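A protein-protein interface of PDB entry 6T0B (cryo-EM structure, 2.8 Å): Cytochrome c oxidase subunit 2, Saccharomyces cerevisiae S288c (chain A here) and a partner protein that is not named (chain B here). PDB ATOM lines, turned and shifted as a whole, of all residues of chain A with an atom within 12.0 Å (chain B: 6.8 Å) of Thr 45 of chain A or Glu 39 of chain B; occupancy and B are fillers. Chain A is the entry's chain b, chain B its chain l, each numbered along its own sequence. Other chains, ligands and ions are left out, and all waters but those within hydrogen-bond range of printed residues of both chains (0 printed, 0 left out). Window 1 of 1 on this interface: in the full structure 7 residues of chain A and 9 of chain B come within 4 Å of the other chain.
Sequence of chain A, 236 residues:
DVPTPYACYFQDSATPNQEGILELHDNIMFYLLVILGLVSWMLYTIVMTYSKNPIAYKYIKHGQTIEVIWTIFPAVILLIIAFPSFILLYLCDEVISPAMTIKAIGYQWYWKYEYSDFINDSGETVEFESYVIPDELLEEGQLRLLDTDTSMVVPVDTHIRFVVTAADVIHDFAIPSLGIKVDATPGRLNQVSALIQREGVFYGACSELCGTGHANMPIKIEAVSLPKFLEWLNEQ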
ATOM      1  N   LEU A  36     -19.312   5.260   5.272  1.00  0.00           N
ATOM      2  CA  LEU A  36     -20.689   5.566   5.634  1.00  0.00           C
ATOM      3  C   LEU A  36     -21.131   4.774   6.848  1.00  0.00           C
ATOM      4  O   LEU A  36     -21.778   5.327   7.743  1.00  0.00           O
ATOM      5  CB  LEU A  36     -21.613   5.283   4.462  1.00  0.00           C
ATOM      6  CG  LEU A  36     -23.101   5.302   4.768  1.00  0.00           C
ATOM      7  CD1 LEU A  36     -23.530   6.707   5.104  1.00  0.00           C
ATOM      8  CD2 LEU A  36     -23.879   4.773   3.599  1.00  0.00           C
ATOM      9  N   GLY A  37     -20.760   3.497   6.915  1.00  0.00           N
ATOM     10  CA  GLY A  37     -21.087   2.705   8.084  1.00  0.00           C
ATOM     11  C   GLY A  37     -20.395   3.198   9.334  1.00  0.00           C
ATOM     12  O   GLY A  37     -20.998   3.232  10.405  1.00  0.00           O
ATOM     13  N   LEU A  38     -19.147   3.651   9.195  1.00  0.00           N
ATOM     14  CA  LEU A  38     -18.424   4.221  10.329  1.00  0.00           C
ATOM     15  C   LEU A  38     -19.095   5.482  10.849  1.00  0.00           C
ATOM     16  O   LEU A  38     -19.408   5.575  12.040  1.00  0.00           O
ATOM     17  CB  LEU A  38     -16.986   4.523   9.939  1.00  0.00           C
ATOM     18  CG  LEU A  38     -16.228   5.326  10.988  1.00  0.00           C
ATOM     19  CD1 LEU A  38     -15.720   4.408  12.059  1.00  0.00           C
ATOM     20  CD2 LEU A  38     -15.090   6.073  10.355  1.00  0.00           C
ATOM     21  N   VAL A  39     -19.348   6.454   9.972  1.00  0.00           N
ATOM     22  CA  VAL A  39     -19.836   7.729  10.479  1.00  0.00           C
ATOM     23  C   VAL A  39     -21.298   7.632  10.877  1.00  0.00           C
ATOM     24  O   VAL A  39     -21.723   8.307  11.815  1.00  0.00           O
ATOM     25  CB  VAL A  39     -19.587   8.873   9.479  1.00  0.00           C
ATOM     26  CG1 VAL A  39     -18.112   9.013   9.202  1.00  0.00           C
ATOM     27  CG2 VAL A  39     -20.341   8.679   8.201  1.00  0.00           C
ATOM     28  N   SER A  40     -22.075   6.744  10.253  1.00  0.00           N
ATOM     29  CA  SER A  40     -23.451   6.569  10.680  1.00  0.00           C
ATOM     30  C   SER A  40     -23.536   5.787  11.974  1.00  0.00           C
ATOM     31  O   SER A  40     -24.416   6.062  12.792  1.00  0.00           O
ATOM     32  CB  SER A  40     -24.257   5.857   9.609  1.00  0.00           C
ATOM     33  OG  SER A  40     -23.809   4.527   9.493  1.00  0.00           O
ATOM     34  N   TRP A  41     -22.612   4.851  12.207  1.00  0.00           N
ATOM     35  CA  TRP A  41     -22.592   4.167  13.489  1.00  0.00           C
ATOM     36  C   TRP A  41     -22.177   5.103  14.611  1.00  0.00           C
ATOM     37  O   TRP A  41     -22.764   5.060  15.696  1.00  0.00           O
ATOM     38  CB  TRP A  41     -21.667   2.960  13.445  1.00  0.00           C
ATOM     39  CG  TRP A  41     -21.325   2.487  14.786  1.00  0.00           C
ATOM     40  CD1 TRP A  41     -20.128   2.591  15.399  1.00  0.00           C
ATOM     41  CD2 TRP A  41     -22.198   1.853  15.715  1.00  0.00           C
ATOM     42  NE1 TRP A  41     -20.188   2.055  16.646  1.00  0.00           N
ATOM     43  CE2 TRP A  41     -21.456   1.593  16.866  1.00  0.00           C
ATOM     44  CE3 TRP A  41     -23.538   1.477  15.683  1.00  0.00           C
ATOM     45  CZ2 TRP A  41     -22.002   0.974  17.979  1.00  0.00           C
ATOM     46  CZ3 TRP A  41     -24.077   0.865  16.789  1.00  0.00           C
ATOM     47  CH2 TRP A  41     -23.312   0.618  17.919  1.00  0.00           C
ATOM     48  N   MET A  42     -21.181   5.963  14.369  1.00  0.00           N
ATOM     49  CA  MET A  42     -20.797   6.943  15.380  1.00  0.00           C
ATOM     50  C   MET A  42     -21.921   7.928  15.640  1.00  0.00           C
ATOM     51  O   MET A  42     -22.236   8.221  16.791  1.00  0.00           O
ATOM     52  CB  MET A  42     -19.542   7.698  14.961  1.00  0.00           C
ATOM     53  CG  MET A  42     -18.304   6.859  14.817  1.00  0.00           C
ATOM     54  SD  MET A  42     -17.893   5.909  16.275  1.00  0.00           S
ATOM     55  CE  MET A  42     -17.671   7.202  17.474  1.00  0.00           C
ATOM     56  N   LEU A  43     -22.555   8.422  14.585  1.00  0.00           N
ATOM     57  CA  LEU A  43     -23.639   9.375  14.743  1.00  0.00           C
ATOM     58  C   LEU A  43     -24.850   8.748  15.408  1.00  0.00           C
ATOM     59  O   LEU A  43     -25.626   9.454  16.053  1.00  0.00           O
ATOM     60  CB  LEU A  43     -24.005   9.948  13.379  1.00  0.00           C
ATOM     61  CG  LEU A  43     -24.776  11.257  13.309  1.00  0.00           C
ATOM     62  CD1 LEU A  43     -24.102  12.322  14.129  1.00  0.00           C
ATOM     63  CD2 LEU A  43     -24.891  11.696  11.879  1.00  0.00           C
ATOM     64  N   TYR A  44     -25.023   7.432  15.297  1.00  0.00           N
ATOM     65  CA  TYR A  44     -26.090   6.794  16.052  1.00  0.00           C
ATOM     66  C   TYR A  44     -25.706   6.619  17.509  1.00  0.00           C
ATOM     67  O   TYR A  44     -26.475   6.985  18.409  1.00  0.00           O
ATOM     68  CB  TYR A  44     -26.454   5.441  15.453  1.00  0.00           C
ATOM     69  CG  TYR A  44     -27.721   4.931  16.057  1.00  0.00           C
ATOM     70  CD1 TYR A  44     -28.937   5.476  15.693  1.00  0.00           C
ATOM     71  CD2 TYR A  44     -27.709   3.952  17.031  1.00  0.00           C
ATOM     72  CE1 TYR A  44     -30.099   5.045  16.258  1.00  0.00           C
ATOM     73  CE2 TYR A  44     -28.871   3.515  17.605  1.00  0.00           C
ATOM     74  CZ  TYR A  44     -30.061   4.070  17.214  1.00  0.00           C
ATOM     75  OH  TYR A  44     -31.243   3.655  17.768  1.00  0.00           O
ATOM     76  N   THR A  45     -24.525   6.059  17.760  1.00  0.00           N
ATOM     77  CA  THR A  45     -24.173   5.692  19.120  1.00  0.00           C
ATOM     78  C   THR A  45     -23.909   6.911  19.985  1.00  0.00           C
ATOM     79  O   THR A  45     -24.220   6.874  21.170  1.00  0.00           O
ATOM     80  CB  THR A  45     -22.986   4.720  19.132  1.00  0.00           C
ATOM     81  OG1 THR A  45     -22.848   4.153  20.433  1.00  0.00           O
ATOM     82  CG2 THR A  45     -21.677   5.371  18.769  1.00  0.00           C
ATOM     83  N   ILE A  46     -23.465   8.026  19.404  1.00  0.00           N
ATOM     84  CA  ILE A  46     -23.162   9.211  20.192  1.00  0.00           C
ATOM     85  C   ILE A  46     -24.445   9.857  20.682  1.00  0.00           C
ATOM     86  O   ILE A  46     -24.598  10.143  21.872  1.00  0.00           O
ATOM     87  CB  ILE A  46     -22.318  10.191  19.367  1.00  0.00           C
ATOM     88  CG1 ILE A  46     -20.883   9.715  19.287  1.00  0.00           C
ATOM     89  CG2 ILE A  46     -22.321  11.543  19.991  1.00  0.00           C
ATOM     90  CD1 ILE A  46     -20.114  10.371  18.197  1.00  0.00           C
ATOM     91  N   VAL A  47     -25.404  10.067  19.783  1.00  0.00           N
ATOM     92  CA  VAL A  47     -26.658  10.670  20.210  1.00  0.00           C
ATOM     93  C   VAL A  47     -27.573   9.683  20.902  1.00  0.00           C
ATOM     94  O   VAL A  47     -28.622  10.091  21.406  1.00  0.00           O
ATOM     95  CB  VAL A  47     -27.442  11.309  19.051  1.00  0.00           C
ATOM     96  CG1 VAL A  47     -26.560  12.244  18.277  1.00  0.00           C
ATOM     97  CG2 VAL A  47     -28.016  10.261  18.158  1.00  0.00           C
ATOM     98  N   MET A  48     -27.231   8.401  20.945  1.00  0.00           N
ATOM     99  CA  MET A  48     -28.029   7.511  21.765  1.00  0.00           C
ATOM    100  C   MET A  48     -27.385   7.156  23.093  1.00  0.00           C
ATOM    101  O   MET A  48     -28.050   6.540  23.928  1.00  0.00           O
ATOM    102  CB  MET A  48     -28.363   6.237  20.997  1.00  0.00           C
ATOM    103  CG  MET A  48     -29.506   6.433  20.035  1.00  0.00           C
ATOM    104  SD  MET A  48     -30.919   7.204  20.837  1.00  0.00           S
ATOM    105  CE  MET A  48     -31.890   7.682  19.417  1.00  0.00           C
ATOM    106  N   THR A  49     -26.120   7.506  23.322  1.00  0.00           N
ATOM    107  CA  THR A  49     -25.564   7.331  24.653  1.00  0.00           C
ATOM    108  C   THR A  49     -25.177   8.626  25.334  1.00  0.00           C
ATOM    109  O   THR A  49     -24.821   8.591  26.515  1.00  0.00           O
ATOM    110  CB  THR A  49     -24.336   6.407  24.646  1.00  0.00           C
ATOM    111  OG1 THR A  49     -24.018   6.060  25.991  1.00  0.00           O
ATOM    112  CG2 THR A  49     -23.136   7.107  24.124  1.00  0.00           C
ATOM    113  N   TYR A  50     -25.243   9.760  24.652  1.00  0.00           N
ATOM    114  CA  TYR A  50     -24.879  11.022  25.261  1.00  0.00           C
ATOM    115  C   TYR A  50     -26.021  12.010  25.271  1.00  0.00           C
ATOM    116  O   TYR A  50     -25.876  13.095  25.829  1.00  0.00           O
ATOM    117  CB  TYR A  50     -23.671  11.608  24.546  1.00  0.00           C
ATOM    118  CG  TYR A  50     -22.449  10.772  24.768  1.00  0.00           C
ATOM    119  CD1 TYR A  50     -22.088  10.381  26.041  1.00  0.00           C
ATOM    120  CD2 TYR A  50     -21.666  10.361  23.711  1.00  0.00           C
ATOM    121  CE1 TYR A  50     -20.987   9.615  26.255  1.00  0.00           C
ATOM    122  CE2 TYR A  50     -20.564   9.592  23.919  1.00  0.00           C
ATOM    123  CZ  TYR A  50     -20.233   9.221  25.193  1.00  0.00           C
ATOM    124  OH  TYR A  50     -19.123   8.451  25.407  1.00  0.00           O
ATOM    125  N   SER A  51     -27.146  11.667  24.656  1.00  0.00           N
ATOM    126  CA  SER A  51     -28.365  12.410  24.902  1.00  0.00           C
ATOM    127  C   SER A  51     -28.818  12.236  26.335  1.00  0.00           C
ATOM    128  O   SER A  51     -29.383  13.164  26.919  1.00  0.00           O
ATOM    129  CB  SER A  51     -29.461  11.953  23.958  1.00  0.00           C
ATOM    130  OG  SER A  51     -29.763  10.596  24.199  1.00  0.00           O
ATOM    131  N   LYS A  52     -28.577  11.064  26.921  1.00  0.00           N
ATOM    132  CA  LYS A  52     -28.899  10.813  28.317  1.00  0.00           C
ATOM    133  C   LYS A  52     -27.668  10.864  29.207  1.00  0.00           C
ATOM    134  O   LYS A  52     -27.603  10.164  30.218  1.00  0.00           O
ATOM    135  CB  LYS A  52     -29.616   9.477  28.471  1.00  0.00           C
ATOM    136  CG  LYS A  52     -29.137   8.385  27.555  1.00  0.00           C
ATOM    137  CD  LYS A  52     -29.935   7.117  27.796  1.00  0.00           C
ATOM    138  CE  LYS A  52     -29.246   5.902  27.218  1.00  0.00           C
ATOM    139  NZ  LYS A  52     -27.923   5.670  27.859  1.00  0.00           N
ATOM    140  N   ASN A  53     -26.693  11.691  28.850  1.00  0.00           N
ATOM    141  CA  ASN A  53     -25.509  11.884  29.663  1.00  0.00           C
ATOM    142  C   ASN A  53     -25.587  13.237  30.334  1.00  0.00           C
ATOM    143  O   ASN A  53     -25.685  14.252  29.635  1.00  0.00           O
ATOM    144  CB  ASN A  53     -24.261  11.793  28.809  1.00  0.00           C
ATOM    145  CG  ASN A  53     -23.036  12.261  29.524  1.00  0.00           C
ATOM    146  OD1 ASN A  53     -22.825  11.949  30.689  1.00  0.00           O
ATOM    147  ND2 ASN A  53     -22.200  13.001  28.822  1.00  0.00           N
ATOM    148  N   TYR A  57     -17.911  15.888  29.212  1.00  0.00           N
ATOM    149  CA  TYR A  57     -16.458  15.862  29.341  1.00  0.00           C
ATOM    150  C   TYR A  57     -15.894  17.092  28.647  1.00  0.00           C
ATOM    151  O   TYR A  57     -15.345  17.025  27.550  1.00  0.00           O
ATOM    152  CB  TYR A  57     -15.890  14.590  28.730  1.00  0.00           C
ATOM    153  CG  TYR A  57     -16.250  13.311  29.439  1.00  0.00           C
ATOM    154  CD1 TYR A  57     -17.448  12.673  29.203  1.00  0.00           C
ATOM    155  CD2 TYR A  57     -15.375  12.737  30.327  1.00  0.00           C
ATOM    156  CE1 TYR A  57     -17.764  11.510  29.850  1.00  0.00           C
ATOM    157  CE2 TYR A  57     -15.681  11.578  30.967  1.00  0.00           C
ATOM    158  CZ  TYR A  57     -16.874  10.969  30.729  1.00  0.00           C
ATOM    159  OH  TYR A  57     -17.167   9.804  31.383  1.00  0.00           O
ATOM    160  N   ARG B  35     -24.363  -3.073  26.801  1.00  0.00           N
ATOM    161  CA  ARG B  35     -24.806  -1.768  26.331  1.00  0.00           C
ATOM    162  C   ARG B  35     -24.733  -1.627  24.815  1.00  0.00           C
ATOM    163  O   ARG B  35     -25.652  -1.086  24.200  1.00  0.00           O
ATOM    164  CB  ARG B  35     -23.967  -0.671  26.987  1.00  0.00           C
ATOM    165  CG  ARG B  35     -24.226   0.718  26.484  1.00  0.00           C
ATOM    166  CD  ARG B  35     -23.165   1.662  26.982  1.00  0.00           C
ATOM    167  NE  ARG B  35     -21.914   1.520  26.252  1.00  0.00           N
ATOM    168  CZ  ARG B  35     -21.651   2.136  25.106  1.00  0.00           C
ATOM    169  NH1 ARG B  35     -22.555   2.929  24.557  1.00  0.00           N
ATOM    170  NH2 ARG B  35     -20.486   1.957  24.507  1.00  0.00           N
ATOM    171  N   LEU B  36     -23.676  -2.135  24.193  1.00  0.00           N
ATOM    172  CA  LEU B  36     -23.466  -1.967  22.769  1.00  0.00           C
ATOM    173  C   LEU B  36     -24.224  -2.961  21.916  1.00  0.00           C
ATOM    174  O   LEU B  36     -24.425  -2.689  20.730  1.00  0.00           O
ATOM    175  CB  LEU B  36     -21.985  -2.088  22.438  1.00  0.00           C
ATOM    176  CG  LEU B  36     -21.169  -0.819  22.592  1.00  0.00           C
ATOM    177  CD1 LEU B  36     -19.763  -1.083  22.150  1.00  0.00           C
ATOM    178  CD2 LEU B  36     -21.781   0.299  21.780  1.00  0.00           C
ATOM    179  N   ILE B  37     -24.626  -4.105  22.457  1.00  0.00           N
ATOM    180  CA  ILE B  37     -25.349  -5.096  21.662  1.00  0.00           C
ATOM    181  C   ILE B  37     -26.733  -4.617  21.210  1.00  0.00           C
ATOM    182  O   ILE B  37     -27.013  -4.751  20.013  1.00  0.00           O
ATOM    183  CB  ILE B  37     -25.402  -6.446  22.400  1.00  0.00           C
ATOM    184  CG1 ILE B  37     -24.098  -7.204  22.186  1.00  0.00           C
ATOM    185  CG2 ILE B  37     -26.538  -7.315  21.920  1.00  0.00           C
ATOM    186  CD1 ILE B  37     -24.006  -8.468  22.974  1.00  0.00           C
ATOM    187  N   PRO B  38     -27.621  -4.038  22.042  1.00  0.00           N
ATOM    188  CA  PRO B  38     -28.910  -3.595  21.481  1.00  0.00           C
ATOM    189  C   PRO B  38     -28.805  -2.404  20.548  1.00  0.00           C
ATOM    190  O   PRO B  38     -29.629  -2.273  19.634  1.00  0.00           O
ATOM    191  CB  PRO B  38     -29.735  -3.240  22.722  1.00  0.00           C
ATOM    192  CG  PRO B  38     -29.069  -3.888  23.824  1.00  0.00           C
ATOM    193  CD  PRO B  38     -27.638  -3.836  23.501  1.00  0.00           C
ATOM    194  N   GLU B  39     -27.813  -1.539  20.735  1.00  0.00           N
ATOM    195  CA  GLU B  39     -27.688  -0.381  19.867  1.00  0.00           C
ATOM    196  C   GLU B  39     -27.168  -0.738  18.488  1.00  0.00           C
ATOM    197  O   GLU B  39     -27.450  -0.006  17.540  1.00  0.00           O
ATOM    198  CB  GLU B  39     -26.798   0.673  20.517  1.00  0.00           C
ATOM    199  CG  GLU B  39     -27.576   1.564  21.461  1.00  0.00           C
ATOM    200  CD  GLU B  39     -26.737   2.635  22.100  1.00  0.00           C
ATOM    201  OE1 GLU B  39     -27.222   3.265  23.057  1.00  0.00           O
ATOM    202  OE2 GLU B  39     -25.602   2.858  21.646  1.00  0.00           O
ATOM    203  N   ILE B  40     -26.457  -1.859  18.350  1.00  0.00           N
ATOM    204  CA  ILE B  40     -26.116  -2.383  17.030  1.00  0.00           C
ATOM    205  C   ILE B  40     -27.381  -2.729  16.258  1.00  0.00           C
ATOM    206  O   ILE B  40     -27.539  -2.361  15.088  1.00  0.00           O
ATOM    207  CB  ILE B  40     -25.194  -3.605  17.165  1.00  0.00           C
ATOM    208  CG1 ILE B  40     -23.780  -3.176  17.514  1.00  0.00           C
ATOM    209  CG2 ILE B  40     -25.153  -4.397  15.891  1.00  0.00           C
ATOM    210  CD1 ILE B  40     -22.876  -4.335  17.832  1.00  0.00           C
ATOM    211  N   PHE B  41     -28.316  -3.410  16.916  1.00  0.00           N
ATOM    212  CA  PHE B  41     -29.553  -3.808  16.259  1.00  0.00           C
ATOM    213  C   PHE B  41     -30.433  -2.605  15.960  1.00  0.00           C
ATOM    214  O   PHE B  41     -31.086  -2.551  14.907  1.00  0.00           O
ATOM    215  CB  PHE B  41     -30.298  -4.814  17.129  1.00  0.00           C
ATOM    216  CG  PHE B  41     -29.703  -6.184  17.107  1.00  0.00           C
ATOM    217  CD1 PHE B  41     -28.664  -6.513  17.949  1.00  0.00           C
ATOM    218  CD2 PHE B  41     -30.182  -7.144  16.245  1.00  0.00           C
ATOM    219  CE1 PHE B  41     -28.108  -7.767  17.929  1.00  0.00           C
ATOM    220  CE2 PHE B  41     -29.629  -8.405  16.223  1.00  0.00           C
ATOM    221  CZ  PHE B  41     -28.592  -8.713  17.068  1.00  0.00           C
ATOM    222  N   GLN B  42     -30.443  -1.623  16.861  1.00  0.00           N
ATOM    223  CA  GLN B  42     -31.215  -0.410  16.614  1.00  0.00           C
ATOM    224  C   GLN B  42     -30.628   0.399  15.467  1.00  0.00           C
ATOM    225  O   GLN B  42     -31.370   0.963  14.654  1.00  0.00           O
ATOM    226  CB  GLN B  42     -31.284   0.430  17.877  1.00  0.00           C
ATOM    227  CG  GLN B  42     -32.245  -0.088  18.898  1.00  0.00           C
ATOM    228  CD  GLN B  42     -32.141   0.650  20.205  1.00  0.00           C
ATOM    229  OE1 GLN B  42     -32.711   0.232  21.210  1.00  0.00           O
ATOM    230  NE2 GLN B  42     -31.411   1.754  20.205  1.00  0.00           N
ATOM    231  N   TRP B  43     -29.301   0.443  15.373  1.00  0.00           N
ATOM    232  CA  TRP B  43     -28.638   1.109  14.263  1.00  0.00           C
ATOM    233  C   TRP B  43     -28.918   0.404  12.952  1.00  0.00           C
ATOM    234  O   TRP B  43     -29.090   1.060  11.925  1.00  0.00           O
ATOM    235  CB  TRP B  43     -27.139   1.160  14.530  1.00  0.00           C
ATOM    236  CG  TRP B  43     -26.298   1.427  13.351  1.00  0.00           C
ATOM    237  CD1 TRP B  43     -25.946   2.637  12.866  1.00  0.00           C
ATOM    238  CD2 TRP B  43     -25.671   0.461  12.515  1.00  0.00           C
ATOM    239  NE1 TRP B  43     -25.148   2.494  11.770  1.00  0.00           N
ATOM    240  CE2 TRP B  43     -24.966   1.161  11.531  1.00  0.00           C
ATOM    241  CE3 TRP B  43     -25.649  -0.932  12.494  1.00  0.00           C
ATOM    242  CZ2 TRP B  43     -24.241   0.520  10.542  1.00  0.00           C
ATOM    243  CZ3 TRP B  43     -24.930  -1.563  11.514  1.00  0.00           C
ATOM    244  CH2 TRP B  43     -24.236  -0.840  10.551  1.00  0.00           C
ATOM    245  N   SER B  44     -28.957  -0.932  12.972  1.00  0.00           N
ATOM    246  CA  SER B  44     -29.283  -1.699  11.775  1.00  0.00           C
ATOM    247  C   SER B  44     -30.691  -1.400  11.298  1.00  0.00           C
ATOM    248  O   SER B  44     -30.914  -1.194  10.098  1.00  0.00           O
ATOM    249  CB  SER B  44     -29.148  -3.187  12.054  1.00  0.00           C
ATOM    250  OG  SER B  44     -30.159  -3.612  12.941  1.00  0.00           O
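The side-chain hydroxyl (OG) of Ser 40 of chain A is in hydrogen-bond range of the indole nitrogen (NE1) of Trp 43 of chain B (3.3 Å). OH of Tyr 44 of chain A lies within hydrogen-bond range of NE2 of Gln 42 of chain B (3.1 Å). OG1 of Thr 45 of chain A sits at hydrogen-bond distance from OE2 of Glu 39 of chain B (3.3 Å). N of Trp 41 of chain A sits close to NE1 of Trp 43 of chain B. O of Met 48 of chain A lies close to OE1 of Glu 39 of chain B (3.5 Å).
O of Leu 36 of chain A sits at hydrogen-bond distance from OG of Ser 40 of chain A, at 2.8 Å. O of Gly 37 of chain A lies within hydrogen-bond range of OG of Ser 40 of chain A (3.2 Å).
Among the printed residues, pairs that only touch across the chains: Trp 41 of chain A with Glu 39 of chain B, Thr 49 of chain A with Arg 35 of chain B, Tyr 44 of chain A with Trp 43 of chain B, Tyr 44 of chain A with Glu 39 of chain B, Trp 41 of chain A with Ile 40 of chain B and Trp 41 of chain A with Leu 36 of chain B.
Of the printed residues of chain B, Ser 40 of chain A touches Trp 43. Of the printed residues of chain B, Trp 41 of chain A touches Leu 36 (3.9 Å), Glu 39 (3.6 Å), Ile 40 (3.8 Å) and Trp 43 (3.5 Å). Of the printed residues of chain B, Tyr 44 of chain A touches Glu 39, Gln 42 and Trp 43. Of the printed residues of chain B, Met 48 of chain A touches Glu 39 (3.5 Å). Printed residues of chain B within 4 Å of Thr 49 of chain A: Arg 35. Ile 37 of chain B touches none of the printed residues of chain A. No residue of chain A comes within 4 Å of Pro 38 of chain B. Of chain A, only Trp 41 (3.6 Å), Tyr 44 (3.8 Å), Thr 45 (3.3 Å) and Met 48 (3.5 Å) come within 4 Å of Glu 39 of chain B. Ile 40 of chain B touches one residue of chain A. The nearest residue of chain A that does not touch Glu 39 of chain B is Thr 49 of chain A (4.4 Å).
Hydrophobic or aromatic side chains of chain A that line the printed part of chain B: Trp 41, Tyr 44 and Met 48. Hydrophobic or aromatic side chains of chain B that line the printed part of chain A: Leu 36, Ile 40 and Trp 43. Among the printed residues, 11 pairs touch across the chains.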
